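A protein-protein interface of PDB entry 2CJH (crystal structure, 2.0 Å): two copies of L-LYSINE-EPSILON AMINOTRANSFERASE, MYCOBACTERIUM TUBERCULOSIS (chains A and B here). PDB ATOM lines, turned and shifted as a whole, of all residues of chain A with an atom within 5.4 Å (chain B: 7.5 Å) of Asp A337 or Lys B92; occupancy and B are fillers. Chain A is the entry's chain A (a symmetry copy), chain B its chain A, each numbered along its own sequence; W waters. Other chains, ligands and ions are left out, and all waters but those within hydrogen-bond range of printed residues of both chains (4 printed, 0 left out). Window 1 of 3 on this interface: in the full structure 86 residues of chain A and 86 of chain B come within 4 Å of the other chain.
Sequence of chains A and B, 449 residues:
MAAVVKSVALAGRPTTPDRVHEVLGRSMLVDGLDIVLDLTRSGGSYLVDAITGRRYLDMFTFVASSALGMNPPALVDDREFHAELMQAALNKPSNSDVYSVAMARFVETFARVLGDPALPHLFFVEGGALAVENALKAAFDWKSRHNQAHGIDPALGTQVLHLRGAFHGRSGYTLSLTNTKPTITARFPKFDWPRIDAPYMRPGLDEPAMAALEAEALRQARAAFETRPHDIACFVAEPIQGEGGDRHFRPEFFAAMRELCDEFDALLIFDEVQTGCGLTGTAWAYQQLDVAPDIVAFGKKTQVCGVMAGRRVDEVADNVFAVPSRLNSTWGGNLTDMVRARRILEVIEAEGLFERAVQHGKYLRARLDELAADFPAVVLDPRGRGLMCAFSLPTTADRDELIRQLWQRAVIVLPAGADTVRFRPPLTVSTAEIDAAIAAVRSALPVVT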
ATOM      1  N   PHE A  62      -8.152 -19.554 -13.590  1.00  0.00           N
ATOM      2  CA  PHE A  62      -9.629 -19.641 -13.610  1.00  0.00           C
ATOM      3  C   PHE A  62     -10.182 -19.234 -14.993  1.00  0.00           C
ATOM      4  O   PHE A  62     -11.058 -18.349 -15.110  1.00  0.00           O
ATOM      5  CB  PHE A  62     -10.274 -18.811 -12.469  1.00  0.00           C
ATOM      6  CG  PHE A  62      -9.784 -19.178 -11.067  1.00  0.00           C
ATOM      7  CD1 PHE A  62      -9.825 -20.517 -10.610  1.00  0.00           C
ATOM      8  CD2 PHE A  62      -9.336 -18.184 -10.193  1.00  0.00           C
ATOM      9  CE1 PHE A  62      -9.401 -20.859  -9.318  1.00  0.00           C
ATOM     10  CE2 PHE A  62      -8.920 -18.506  -8.908  1.00  0.00           C
ATOM     11  CZ  PHE A  62      -8.943 -19.864  -8.471  1.00  0.00           C
ATOM     12  N   SER A  65      -9.472 -15.533 -15.897  1.00  0.00           N
ATOM     13  CA  SER A  65     -10.276 -14.523 -15.209  1.00  0.00           C
ATOM     14  C   SER A  65      -9.619 -13.898 -13.951  1.00  0.00           C
ATOM     15  O   SER A  65     -10.224 -13.042 -13.293  1.00  0.00           O
ATOM     16  CB  SER A  65     -11.690 -15.048 -14.876  1.00  0.00           C
ATOM     17  OG  SER A  65     -11.686 -15.870 -13.704  1.00  0.00           O
ATOM     18  N   PHE A 106     -15.635   2.485  -7.715  1.00  0.00           N
ATOM     19  CA  PHE A 106     -15.278   1.518  -8.748  1.00  0.00           C
ATOM     20  C   PHE A 106     -15.407   2.151 -10.140  1.00  0.00           C
ATOM     21  O   PHE A 106     -14.509   2.019 -10.986  1.00  0.00           O
ATOM     22  CB  PHE A 106     -16.124   0.248  -8.662  1.00  0.00           C
ATOM     23  CG  PHE A 106     -16.184  -0.515  -9.953  1.00  0.00           C
ATOM     24  CD1 PHE A 106     -15.094  -1.283 -10.386  1.00  0.00           C
ATOM     25  CD2 PHE A 106     -17.303  -0.435 -10.761  1.00  0.00           C
ATOM     26  CE1 PHE A 106     -15.148  -1.982 -11.617  1.00  0.00           C
ATOM     27  CE2 PHE A 106     -17.363  -1.123 -11.990  1.00  0.00           C
ATOM     28  CZ  PHE A 106     -16.296  -1.911 -12.404  1.00  0.00           C
ATOM     29  N   THR A 302     -11.955  -8.422 -15.281  1.00  0.00           N
ATOM     30  CA  THR A 302     -12.632  -7.255 -14.707  1.00  0.00           C
ATOM     31  C   THR A 302     -13.604  -7.647 -13.559  1.00  0.00           C
ATOM     32  O   THR A 302     -14.108  -6.762 -12.876  1.00  0.00           O
ATOM     33  CB  THR A 302     -13.399  -6.435 -15.803  1.00  0.00           C
ATOM     34  OG1 THR A 302     -14.444  -7.243 -16.370  1.00  0.00           O
ATOM     35  CG2 THR A 302     -12.469  -5.982 -16.918  1.00  0.00           C
ATOM     36  N   GLN A 303     -13.883  -8.948 -13.388  1.00  0.00           N
ATOM     37  CA  GLN A 303     -14.746  -9.491 -12.293  1.00  0.00           C
ATOM     38  C   GLN A 303     -16.234  -9.144 -12.518  1.00  0.00           C
ATOM     39  O   GLN A 303     -17.066 -10.044 -12.673  1.00  0.00           O
ATOM     40  CB  GLN A 303     -14.248  -9.077 -10.878  1.00  0.00           C
ATOM     41  CG  GLN A 303     -12.732  -9.336 -10.652  1.00  0.00           C
ATOM     42  CD  GLN A 303     -12.469 -10.792 -10.424  1.00  0.00           C
ATOM     43  OE1 GLN A 303     -12.595 -11.272  -9.302  1.00  0.00           O
ATOM     44  NE2 GLN A 303     -12.121 -11.529 -11.500  1.00  0.00           N
ATOM     45  N   VAL A 304     -16.544  -7.851 -12.549  1.00  0.00           N
ATOM     46  CA  VAL A 304     -17.826  -7.348 -13.102  1.00  0.00           C
ATOM     47  C   VAL A 304     -17.732  -7.323 -14.620  1.00  0.00           C
ATOM     48  O   VAL A 304     -16.673  -6.964 -15.183  1.00  0.00           O
ATOM     49  CB  VAL A 304     -18.136  -5.837 -12.755  1.00  0.00           C
ATOM     50  CG1 VAL A 304     -19.654  -5.632 -12.685  1.00  0.00           C
ATOM     51  CG2 VAL A 304     -17.438  -5.377 -11.537  1.00  0.00           C
ATOM     52  N   ASN A 334     -22.299  -7.345  -9.587  1.00  0.00           N
ATOM     53  CA  ASN A 334     -22.141  -7.727  -8.216  1.00  0.00           C
ATOM     54  C   ASN A 334     -21.293  -6.665  -7.504  1.00  0.00           C
ATOM     55  O   ASN A 334     -20.138  -6.432  -7.882  1.00  0.00           O
ATOM     56  CB  ASN A 334     -21.460  -9.104  -8.164  1.00  0.00           C
ATOM     57  CG  ASN A 334     -21.636  -9.784  -6.834  1.00  0.00           C
ATOM     58  OD1 ASN A 334     -21.413  -9.179  -5.792  1.00  0.00           O
ATOM     59  ND2 ASN A 334     -22.099 -11.031  -6.855  1.00  0.00           N
ATOM     60  N   LEU A 335     -21.845  -6.032  -6.469  1.00  0.00           N
ATOM     61  CA  LEU A 335     -21.106  -4.982  -5.735  1.00  0.00           C
ATOM     62  C   LEU A 335     -19.771  -5.502  -5.146  1.00  0.00           C
ATOM     63  O   LEU A 335     -18.777  -4.786  -5.161  1.00  0.00           O
ATOM     64  CB  LEU A 335     -21.947  -4.363  -4.606  1.00  0.00           C
ATOM     65  CG  LEU A 335     -21.308  -3.179  -3.859  1.00  0.00           C
ATOM     66  CD1 LEU A 335     -20.975  -2.005  -4.833  1.00  0.00           C
ATOM     67  CD2 LEU A 335     -22.232  -2.705  -2.749  1.00  0.00           C
ATOM     68  N   THR A 336     -19.752  -6.748  -4.666  1.00  0.00           N
ATOM     69  CA  THR A 336     -18.513  -7.361  -4.178  1.00  0.00           C
ATOM     70  C   THR A 336     -17.439  -7.418  -5.270  1.00  0.00           C
ATOM     71  O   THR A 336     -16.272  -7.109  -5.017  1.00  0.00           O
ATOM     72  CB  THR A 336     -18.773  -8.783  -3.630  1.00  0.00           C
ATOM     73  OG1 THR A 336     -19.687  -8.695  -2.540  1.00  0.00           O
ATOM     74  CG2 THR A 336     -17.483  -9.444  -3.077  1.00  0.00           C
ATOM     75  N   ASP A 337     -17.844  -7.802  -6.482  1.00  0.00           N
ATOM     76  CA  ASP A 337     -16.927  -7.794  -7.637  1.00  0.00           C
ATOM     77  C   ASP A 337     -16.400  -6.406  -8.005  1.00  0.00           C
ATOM     78  O   ASP A 337     -15.246  -6.277  -8.412  1.00  0.00           O
ATOM     79  CB  ASP A 337     -17.601  -8.411  -8.883  1.00  0.00           C
ATOM     80  CG  ASP A 337     -17.800  -9.931  -8.754  1.00  0.00           C
ATOM     81  OD1 ASP A 337     -17.190 -10.590  -7.890  1.00  0.00           O
ATOM     82  OD2 ASP A 337     -18.570 -10.467  -9.533  1.00  0.00           O
ATOM     83  N   MET A 338     -17.250  -5.387  -7.896  1.00  0.00           N
ATOM     84  CA  MET A 338     -16.846  -3.990  -8.158  1.00  0.00           C
ATOM     85  C   MET A 338     -15.807  -3.517  -7.168  1.00  0.00           C
ATOM     86  O   MET A 338     -14.827  -2.872  -7.547  1.00  0.00           O
ATOM     87  CB  MET A 338     -18.050  -3.056  -8.047  1.00  0.00           C
ATOM     88  CG  MET A 338     -19.094  -3.261  -9.169  1.00  0.00           C
ATOM     89  SD  MET A 338     -20.519  -2.170  -8.981  1.00  0.00           S
ATOM     90  CE  MET A 338     -19.637  -0.677  -8.691  1.00  0.00           C
ATOM     91  N   VAL A 339     -16.031  -3.807  -5.885  1.00  0.00           N
ATOM     92  CA  VAL A 339     -15.061  -3.405  -4.855  1.00  0.00           C
ATOM     93  C   VAL A 339     -13.686  -4.143  -5.026  1.00  0.00           C
ATOM     94  O   VAL A 339     -12.625  -3.513  -4.921  1.00  0.00           O
ATOM     95  CB  VAL A 339     -15.654  -3.593  -3.422  1.00  0.00           C
ATOM     96  CG1 VAL A 339     -14.581  -3.311  -2.352  1.00  0.00           C
ATOM     97  CG2 VAL A 339     -16.903  -2.695  -3.219  1.00  0.00           C
ATOM     98  N   ARG A 340     -13.711  -5.463  -5.294  1.00  0.00           N
ATOM     99  CA  ARG A 340     -12.486  -6.231  -5.594  1.00  0.00           C
ATOM    100  C   ARG A 340     -11.776  -5.689  -6.850  1.00  0.00           C
ATOM    101  O   ARG A 340     -10.540  -5.483  -6.851  1.00  0.00           O
ATOM    102  CB  ARG A 340     -12.788  -7.728  -5.818  1.00  0.00           C
ATOM    103  CG  ARG A 340     -11.562  -8.636  -5.602  1.00  0.00           C
ATOM    104  CD  ARG A 340     -11.930 -10.158  -5.489  1.00  0.00           C
ATOM    105  NE  ARG A 340     -12.840 -10.457  -6.506  1.00  0.00           N
ATOM    106  CZ  ARG A 340     -14.120 -10.794  -6.406  1.00  0.00           C
ATOM    107  NH1 ARG A 340     -14.785 -11.069  -5.267  1.00  0.00           N
ATOM    108  NH2 ARG A 340     -14.689 -10.932  -7.557  1.00  0.00           N
ATOM    109  N   ALA A 341     -12.553  -5.482  -7.914  1.00  0.00           N
ATOM    110  CA  ALA A 341     -12.039  -4.982  -9.176  1.00  0.00           C
ATOM    111  C   ALA A 341     -11.427  -3.613  -9.006  1.00  0.00           C
ATOM    112  O   ALA A 341     -10.357  -3.351  -9.565  1.00  0.00           O
ATOM    113  CB  ALA A 341     -13.147  -4.943 -10.276  1.00  0.00           C
ATOM    114  N   ARG A 342     -12.070  -2.750  -8.208  1.00  0.00           N
ATOM    115  CA  ARG A 342     -11.500  -1.426  -7.933  1.00  0.00           C
ATOM    116  C   ARG A 342     -10.079  -1.545  -7.357  1.00  0.00           C
ATOM    117  O   ARG A 342      -9.117  -0.895  -7.840  1.00  0.00           O
ATOM    118  CB  ARG A 342     -12.351  -0.580  -6.975  1.00  0.00           C
ATOM    119  CG  ARG A 342     -11.501   0.654  -6.612  1.00  0.00           C
ATOM    120  CD  ARG A 342     -11.839   1.492  -5.449  1.00  0.00           C
ATOM    121  NE  ARG A 342     -12.298   0.821  -4.245  1.00  0.00           N
ATOM    122  CZ  ARG A 342     -11.568   0.570  -3.166  1.00  0.00           C
ATOM    123  NH1 ARG A 342     -10.269   0.878  -3.113  1.00  0.00           N
ATOM    124  NH2 ARG A 342     -12.159   0.006  -2.129  1.00  0.00           N
ATOM    125  N   GLN B  87     -12.732 -15.158   3.042  1.00  0.00           N
ATOM    126  CA  GLN B  87     -12.000 -16.122   2.233  1.00  0.00           C
ATOM    127  C   GLN B  87     -12.572 -16.247   0.841  1.00  0.00           C
ATOM    128  O   GLN B  87     -11.819 -16.343  -0.123  1.00  0.00           O
ATOM    129  CB  GLN B  87     -12.007 -17.520   2.872  1.00  0.00           C
ATOM    130  CG  GLN B  87     -11.007 -17.711   3.995  1.00  0.00           C
ATOM    131  CD  GLN B  87     -11.146 -19.071   4.698  1.00  0.00           C
ATOM    132  OE1 GLN B  87     -10.953 -19.153   5.929  1.00  0.00           O
ATOM    133  NE2 GLN B  87     -11.497 -20.141   3.931  1.00  0.00           N
ATOM    134  N   ALA B  88     -13.903 -16.288   0.735  1.00  0.00           N
ATOM    135  CA  ALA B  88     -14.568 -16.381  -0.576  1.00  0.00           C
ATOM    136  C   ALA B  88     -14.465 -15.087  -1.362  1.00  0.00           C
ATOM    137  O   ALA B  88     -14.255 -15.105  -2.573  1.00  0.00           O
ATOM    138  CB  ALA B  88     -16.024 -16.761  -0.390  1.00  0.00           C
ATOM    139  N   ALA B  89     -14.637 -13.961  -0.664  1.00  0.00           N
ATOM    140  CA  ALA B  89     -14.755 -12.663  -1.299  1.00  0.00           C
ATOM    141  C   ALA B  89     -13.458 -12.144  -1.907  1.00  0.00           C
ATOM    142  O   ALA B  89     -13.504 -11.386  -2.855  1.00  0.00           O
ATOM    143  CB  ALA B  89     -15.344 -11.607  -0.306  1.00  0.00           C
ATOM    144  N   LEU B  90     -12.317 -12.531  -1.341  1.00  0.00           N
ATOM    145  CA  LEU B  90     -11.028 -12.052  -1.829  1.00  0.00           C
ATOM    146  C   LEU B  90     -10.726 -12.498  -3.246  1.00  0.00           C
ATOM    147  O   LEU B  90     -10.095 -11.765  -4.003  1.00  0.00           O
ATOM    148  CB  LEU B  90      -9.877 -12.451  -0.882  1.00  0.00           C
ATOM    149  CG  LEU B  90      -9.697 -11.575   0.378  1.00  0.00           C
ATOM    150  CD1 LEU B  90      -8.841 -12.345   1.424  1.00  0.00           C
ATOM    151  CD2 LEU B  90      -9.062 -10.224   0.069  1.00  0.00           C
ATOM    152  N   ASN B  91     -11.188 -13.682  -3.622  1.00  0.00           N
ATOM    153  CA  ASN B  91     -10.917 -14.204  -4.966  1.00  0.00           C
ATOM    154  C   ASN B  91     -12.245 -14.549  -5.669  1.00  0.00           C
ATOM    155  O   ASN B  91     -13.326 -14.418  -5.088  1.00  0.00           O
ATOM    156  CB  ASN B  91      -9.983 -15.435  -4.868  1.00  0.00           C
ATOM    157  CG  ASN B  91      -8.781 -15.179  -3.964  1.00  0.00           C
ATOM    158  OD1 ASN B  91      -7.771 -14.559  -4.384  1.00  0.00           O
ATOM    159  ND2 ASN B  91      -8.893 -15.617  -2.709  1.00  0.00           N
ATOM    160  N   LYS B  92     -12.176 -14.970  -6.910  1.00  0.00           N
ATOM    161  CA  LYS B  92     -13.385 -15.400  -7.628  1.00  0.00           C
ATOM    162  C   LYS B  92     -13.039 -16.616  -8.478  1.00  0.00           C
ATOM    163  O   LYS B  92     -12.784 -16.487  -9.681  1.00  0.00           O
ATOM    164  CB  LYS B  92     -13.988 -14.262  -8.486  1.00  0.00           C
ATOM    165  CG  LYS B  92     -15.366 -14.602  -9.114  1.00  0.00           C
ATOM    166  CD  LYS B  92     -15.968 -13.425  -9.893  1.00  0.00           C
ATOM    167  CE  LYS B  92     -17.450 -13.706 -10.169  1.00  0.00           C
ATOM    168  NZ  LYS B  92     -18.103 -12.640 -10.995  1.00  0.00           N
ATOM    169  N   PRO B  93     -13.019 -17.815  -7.856  1.00  0.00           N
ATOM    170  CA  PRO B  93     -12.700 -19.062  -8.577  1.00  0.00           C
ATOM    171  C   PRO B  93     -13.732 -19.376  -9.661  1.00  0.00           C
ATOM    172  O   PRO B  93     -14.892 -18.959  -9.557  1.00  0.00           O
ATOM    173  CB  PRO B  93     -12.778 -20.137  -7.474  1.00  0.00           C
ATOM    174  CG  PRO B  93     -12.605 -19.364  -6.159  1.00  0.00           C
ATOM    175  CD  PRO B  93     -13.294 -18.052  -6.423  1.00  0.00           C
ATOM    176  N   SER B  94     -13.325 -20.073 -10.709  1.00  0.00           N
ATOM    177  CA  SER B  94     -14.316 -20.639 -11.622  1.00  0.00           C
ATOM    178  C   SER B  94     -14.780 -21.975 -11.025  1.00  0.00           C
ATOM    179  O   SER B  94     -14.089 -22.985 -11.157  1.00  0.00           O
ATOM    180  CB  SER B  94     -13.696 -20.869 -12.988  1.00  0.00           C
ATOM    181  OG  SER B  94     -12.422 -21.477 -12.820  1.00  0.00           O
ATOM    182  N   ASN B  95     -15.924 -21.965 -10.345  1.00  0.00           N
ATOM    183  CA  ASN B  95     -16.499 -23.155  -9.719  1.00  0.00           C
ATOM    184  C   ASN B  95     -16.911 -24.241 -10.717  1.00  0.00           C
ATOM    185  O   ASN B  95     -17.164 -25.384 -10.313  1.00  0.00           O
ATOM    186  CB  ASN B  95     -17.720 -22.780  -8.868  1.00  0.00           C
ATOM    187  CG  ASN B  95     -17.432 -21.644  -7.920  1.00  0.00           C
ATOM    188  OD1 ASN B  95     -16.488 -21.704  -7.097  1.00  0.00           O
ATOM    189  ND2 ASN B  95     -18.231 -20.584  -8.027  1.00  0.00           N
ATOM    190  N   GLU B 126     -24.522 -17.122 -12.732  1.00  0.00           N
ATOM    191  CA  GLU B 126     -24.834 -15.741 -12.318  1.00  0.00           C
ATOM    192  C   GLU B 126     -25.979 -15.234 -13.184  1.00  0.00           C
ATOM    193  O   GLU B 126     -25.878 -15.273 -14.398  1.00  0.00           O
ATOM    194  CB  GLU B 126     -23.628 -14.821 -12.558  1.00  0.00           C
ATOM    195  CG  GLU B 126     -22.391 -15.113 -11.662  1.00  0.00           C
ATOM    196  CD  GLU B 126     -21.277 -14.045 -11.817  1.00  0.00           C
ATOM    197  OE1 GLU B 126     -21.018 -13.555 -12.944  1.00  0.00           O
ATOM    198  OE2 GLU B 126     -20.677 -13.688 -10.793  1.00  0.00           O
ATOM    199  N   THR B 330     -18.277 -19.290 -17.370  1.00  0.00           N
ATOM    200  CA  THR B 330     -16.922 -19.159 -16.796  1.00  0.00           C
ATOM    201  C   THR B 330     -16.907 -19.439 -15.297  1.00  0.00           C
ATOM    202  O   THR B 330     -16.167 -20.312 -14.849  1.00  0.00           O
ATOM    203  CB  THR B 330     -16.226 -17.801 -17.100  1.00  0.00           C
ATOM    204  OG1 THR B 330     -16.008 -17.693 -18.527  1.00  0.00           O
ATOM    205  CG2 THR B 330     -14.856 -17.712 -16.375  1.00  0.00           C
ATOM    206  N   TRP B 331     -17.708 -18.739 -14.511  1.00  0.00           N
ATOM    207  CA  TRP B 331     -17.535 -18.879 -13.065  1.00  0.00           C
ATOM    208  C   TRP B 331     -18.399 -19.961 -12.399  1.00  0.00           C
ATOM    209  O   TRP B 331     -18.057 -20.418 -11.294  1.00  0.00           O
ATOM    210  CB  TRP B 331     -17.739 -17.542 -12.358  1.00  0.00           C
ATOM    211  CG  TRP B 331     -16.602 -16.553 -12.605  1.00  0.00           C
ATOM    212  CD1 TRP B 331     -15.291 -16.676 -12.214  1.00  0.00           C
ATOM    213  CD2 TRP B 331     -16.711 -15.283 -13.282  1.00  0.00           C
ATOM    214  NE1 TRP B 331     -14.574 -15.550 -12.616  1.00  0.00           N
ATOM    215  CE2 TRP B 331     -15.426 -14.685 -13.266  1.00  0.00           C
ATOM    216  CE3 TRP B 331     -17.781 -14.588 -13.882  1.00  0.00           C
ATOM    217  CZ2 TRP B 331     -15.180 -13.414 -13.818  1.00  0.00           C
ATOM    218  CZ3 TRP B 331     -17.522 -13.318 -14.459  1.00  0.00           C
ATOM    219  CH2 TRP B 331     -16.238 -12.758 -14.411  1.00  0.00           C
ATOM    220  N   GLY B 333     -21.418 -19.403 -11.242  1.00  0.00           N
ATOM    221  CA  GLY B 333     -21.955 -18.736 -10.075  1.00  0.00           C
ATOM    222  C   GLY B 333     -20.854 -18.082  -9.253  1.00  0.00           C
ATOM    223  O   GLY B 333     -19.682 -18.439  -9.349  1.00  0.00           O
ATOM    224  N   ASN B 334     -21.235 -17.103  -8.449  1.00  0.00           N
ATOM    225  CA  ASN B 334     -20.296 -16.351  -7.671  1.00  0.00           C
ATOM    226  C   ASN B 334     -20.094 -17.060  -6.324  1.00  0.00           C
ATOM    227  O   ASN B 334     -21.051 -17.225  -5.557  1.00  0.00           O
ATOM    228  CB  ASN B 334     -20.850 -14.931  -7.472  1.00  0.00           C
ATOM    229  CG  ASN B 334     -19.784 -13.951  -7.060  1.00  0.00           C
ATOM    230  OD1 ASN B 334     -19.012 -14.219  -6.149  1.00  0.00           O
ATOM    231  ND2 ASN B 334     -19.695 -12.830  -7.771  1.00  0.00           N
ATOM    232  N   LEU B 335     -18.860 -17.462  -6.023  1.00  0.00           N
ATOM    233  CA  LEU B 335     -18.577 -18.166  -4.754  1.00  0.00           C
ATOM    234  C   LEU B 335     -18.980 -17.331  -3.512  1.00  0.00           C
ATOM    235  O   LEU B 335     -19.486 -17.884  -2.544  1.00  0.00           O
ATOM    236  CB  LEU B 335     -17.099 -18.570  -4.632  1.00  0.00           C
ATOM    237  CG  LEU B 335     -16.728 -19.412  -3.399  1.00  0.00           C
ATOM    238  CD1 LEU B 335     -17.537 -20.747  -3.359  1.00  0.00           C
ATOM    239  CD2 LEU B 335     -15.234 -19.694  -3.392  1.00  0.00           C
ATOM    240  N   THR B 336     -18.780 -16.011  -3.566  1.00  0.00           N
ATOM    241  CA  THR B 336     -19.217 -15.128  -2.481  1.00  0.00           C
ATOM    242  C   THR B 336     -20.729 -15.219  -2.247  1.00  0.00           C
ATOM    243  O   THR B 336     -21.183 -15.286  -1.102  1.00  0.00           O
ATOM    244  CB  THR B 336     -18.822 -13.660  -2.764  1.00  0.00           C
ATOM    245  OG1 THR B 336     -17.403 -13.577  -2.863  1.00  0.00           O
ATOM    246  CG2 THR B 336     -19.245 -12.706  -1.616  1.00  0.00           C
ATOM    247  N   ASP B 337     -21.499 -15.232  -3.338  1.00  0.00           N
ATOM    248  CA  ASP B 337     -22.958 -15.423  -3.247  1.00  0.00           C
ATOM    249  C   ASP B 337     -23.375 -16.774  -2.661  1.00  0.00           C
ATOM    250  O   ASP B 337     -24.367 -16.848  -1.938  1.00  0.00           O
ATOM    251  CB  ASP B 337     -23.626 -15.258  -4.631  1.00  0.00           C
ATOM    252  CG  ASP B 337     -23.612 -13.801  -5.122  1.00  0.00           C
ATOM    253  OD1 ASP B 337     -23.383 -12.859  -4.341  1.00  0.00           O
ATOM    254  OD2 ASP B 337     -23.841 -13.603  -6.303  1.00  0.00           O
HETATM  255  O   HOH W   1     -17.406 -12.359  -5.927  1.00  0.00           O
HETATM  256  O   HOH W   2     -19.917 -10.959 -13.222  1.00  0.00           O
HETATM  257  O   HOH W   3     -21.942 -10.676  -3.903  1.00  0.00           O
HETATM  258  O   HOH W   4     -11.572 -14.616 -11.163  1.00  0.00           O
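OD2 of Asp B337 is in hydrogen-bond range of ND2 of Asn A334 (3.2 Å). NE1 of Trp B331 sits at hydrogen-bond distance from OG of Ser A65. The side-chain carboxylate of Asp A337 is in salt-bridge range of the side-chain amino group of Lys B92. The side-chain amino group (NZ) of Lys B92 is in hydrogen-bond range of the backbone carbonyl oxygen (O) of Gln A303, 3.3 Å away. The backbone carbonyl oxygen of Ala B89 is in hydrogen-bond range of the guanidinium group of Arg A340, at 2.7 Å. The side-chain carboxylate of Asp A337 sits at hydrogen-bond distance from the side-chain amide nitrogen of Asn B334 (3.2 Å). The side-chain amide nitrogen of Asn B334 lies close to the side-chain amide nitrogen of Asn A334 (3.1 Å).
The backbone carbonyl oxygen of Phe A62 lies within hydrogen-bond range of the side-chain hydroxyl of Ser A65 (2.9 Å). The backbone carbonyl oxygen of Ser A65 is in hydrogen-bond range of the side-chain amide nitrogen of Gln A303 (3.0 Å). The side-chain amide oxygen (OE1) of Gln A303 lies within hydrogen-bond range of the guanidinium group (NH2) of Arg A340, 2.7 Å away. N of Asn B95 sits at hydrogen-bond distance from O of Trp B331, at 2.8 Å. OE2 of Glu B126 sits at hydrogen-bond distance from ND2 of Asn B334. The side-chain amino group (NZ) of Lys B92 is in salt-bridge range of the side-chain carboxylate (OE2) of Glu B126, at 2.8 Å.
Lys B92 touches Phe A62. Phe A62 touches Pro B93. Phe A62 touches Ser B94. Trp B331 touches Gln A303. Thr B336 touches Thr A336. Arg A340 touches Leu B90. NH1 of Arg A340 touches O of Asn B91, 3.7 Å away. Lys B92 touches Arg A340.
Of the printed residues of chain B, Gln A303 touches Lys B92 (3.3 Å) and Trp B331 (3.3 Å). Asp A337 touches just these residues of chain B: Lys B92 (2.7 Å) and Asn B334 (3.2 Å). Of the printed residues of chain A, Asn B91 touches Arg A340. Of the printed residues of chain A, Lys B92 touches Phe A62, Gln A303, Asp A337 and Arg A340. Glu B126 touches none of the printed residues of chain A. Printed residues of chain A within 4 Å of Trp B331: Ser A65 and Gln A303. Leu B335 touches none of the printed residues of chain A. The nearest printed residue of chain A that does not touch Asp B337 is Thr A336 (5.9 Å).
Hydrophobic or aromatic side chains of chain A that line the printed part of chain B: Phe A62. Among the printed residues, 15 pairs touch across the chains. Among the printed residues, Asp or Glu carboxylates within 4 Å of a Lys or Arg side-chain nitrogen of the other chain: Asp A337 with Lys B92 (2.7 Å).
Asn A334 touches its own counterpart, Asn B334. Asn A334 touches Asp B337, and with the chains exchanged Asp A337 touches Asn B334. Thr A336 touches its own counterpart, Thr B336. Of the 15 pairs that touch across the chains among the printed residues, 4 have their exchanged pair printed and touching as well.
Water W1 lies within hydrogen-bond range of the side-chain amide oxygen (OD1) of Asn B334 (2.5 Å), the side-chain carboxylate (OD1) of Asp A337 (2.7 Å), the guanidinium group (NH1) of Arg A340 (3.0 Å) and the side-chain hydroxyl (OG1) of Thr B336 (3.3 Å). Water W3 lies within hydrogen-bond range of the side-chain amide oxygen of Asn A334 (2.5 Å), the side-chain carboxylate of Asp B337 (2.7 Å) and the side-chain hydroxyl of Thr A336 (3.3 Å). Water W4 lies within hydrogen-bond range of O of Lys B92 (2.7 Å), OG of Ser A65 (2.8 Å), NE2 of Gln A303 (3.2 Å) and NE1 of Trp B331 (3.5 Å). Water W2 lies within hydrogen-bond range of OE1 of Glu B126 (2.8 Å), O of Gln A303 (3.0 Å) and NZ of Lys B92 (3.3 Å).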
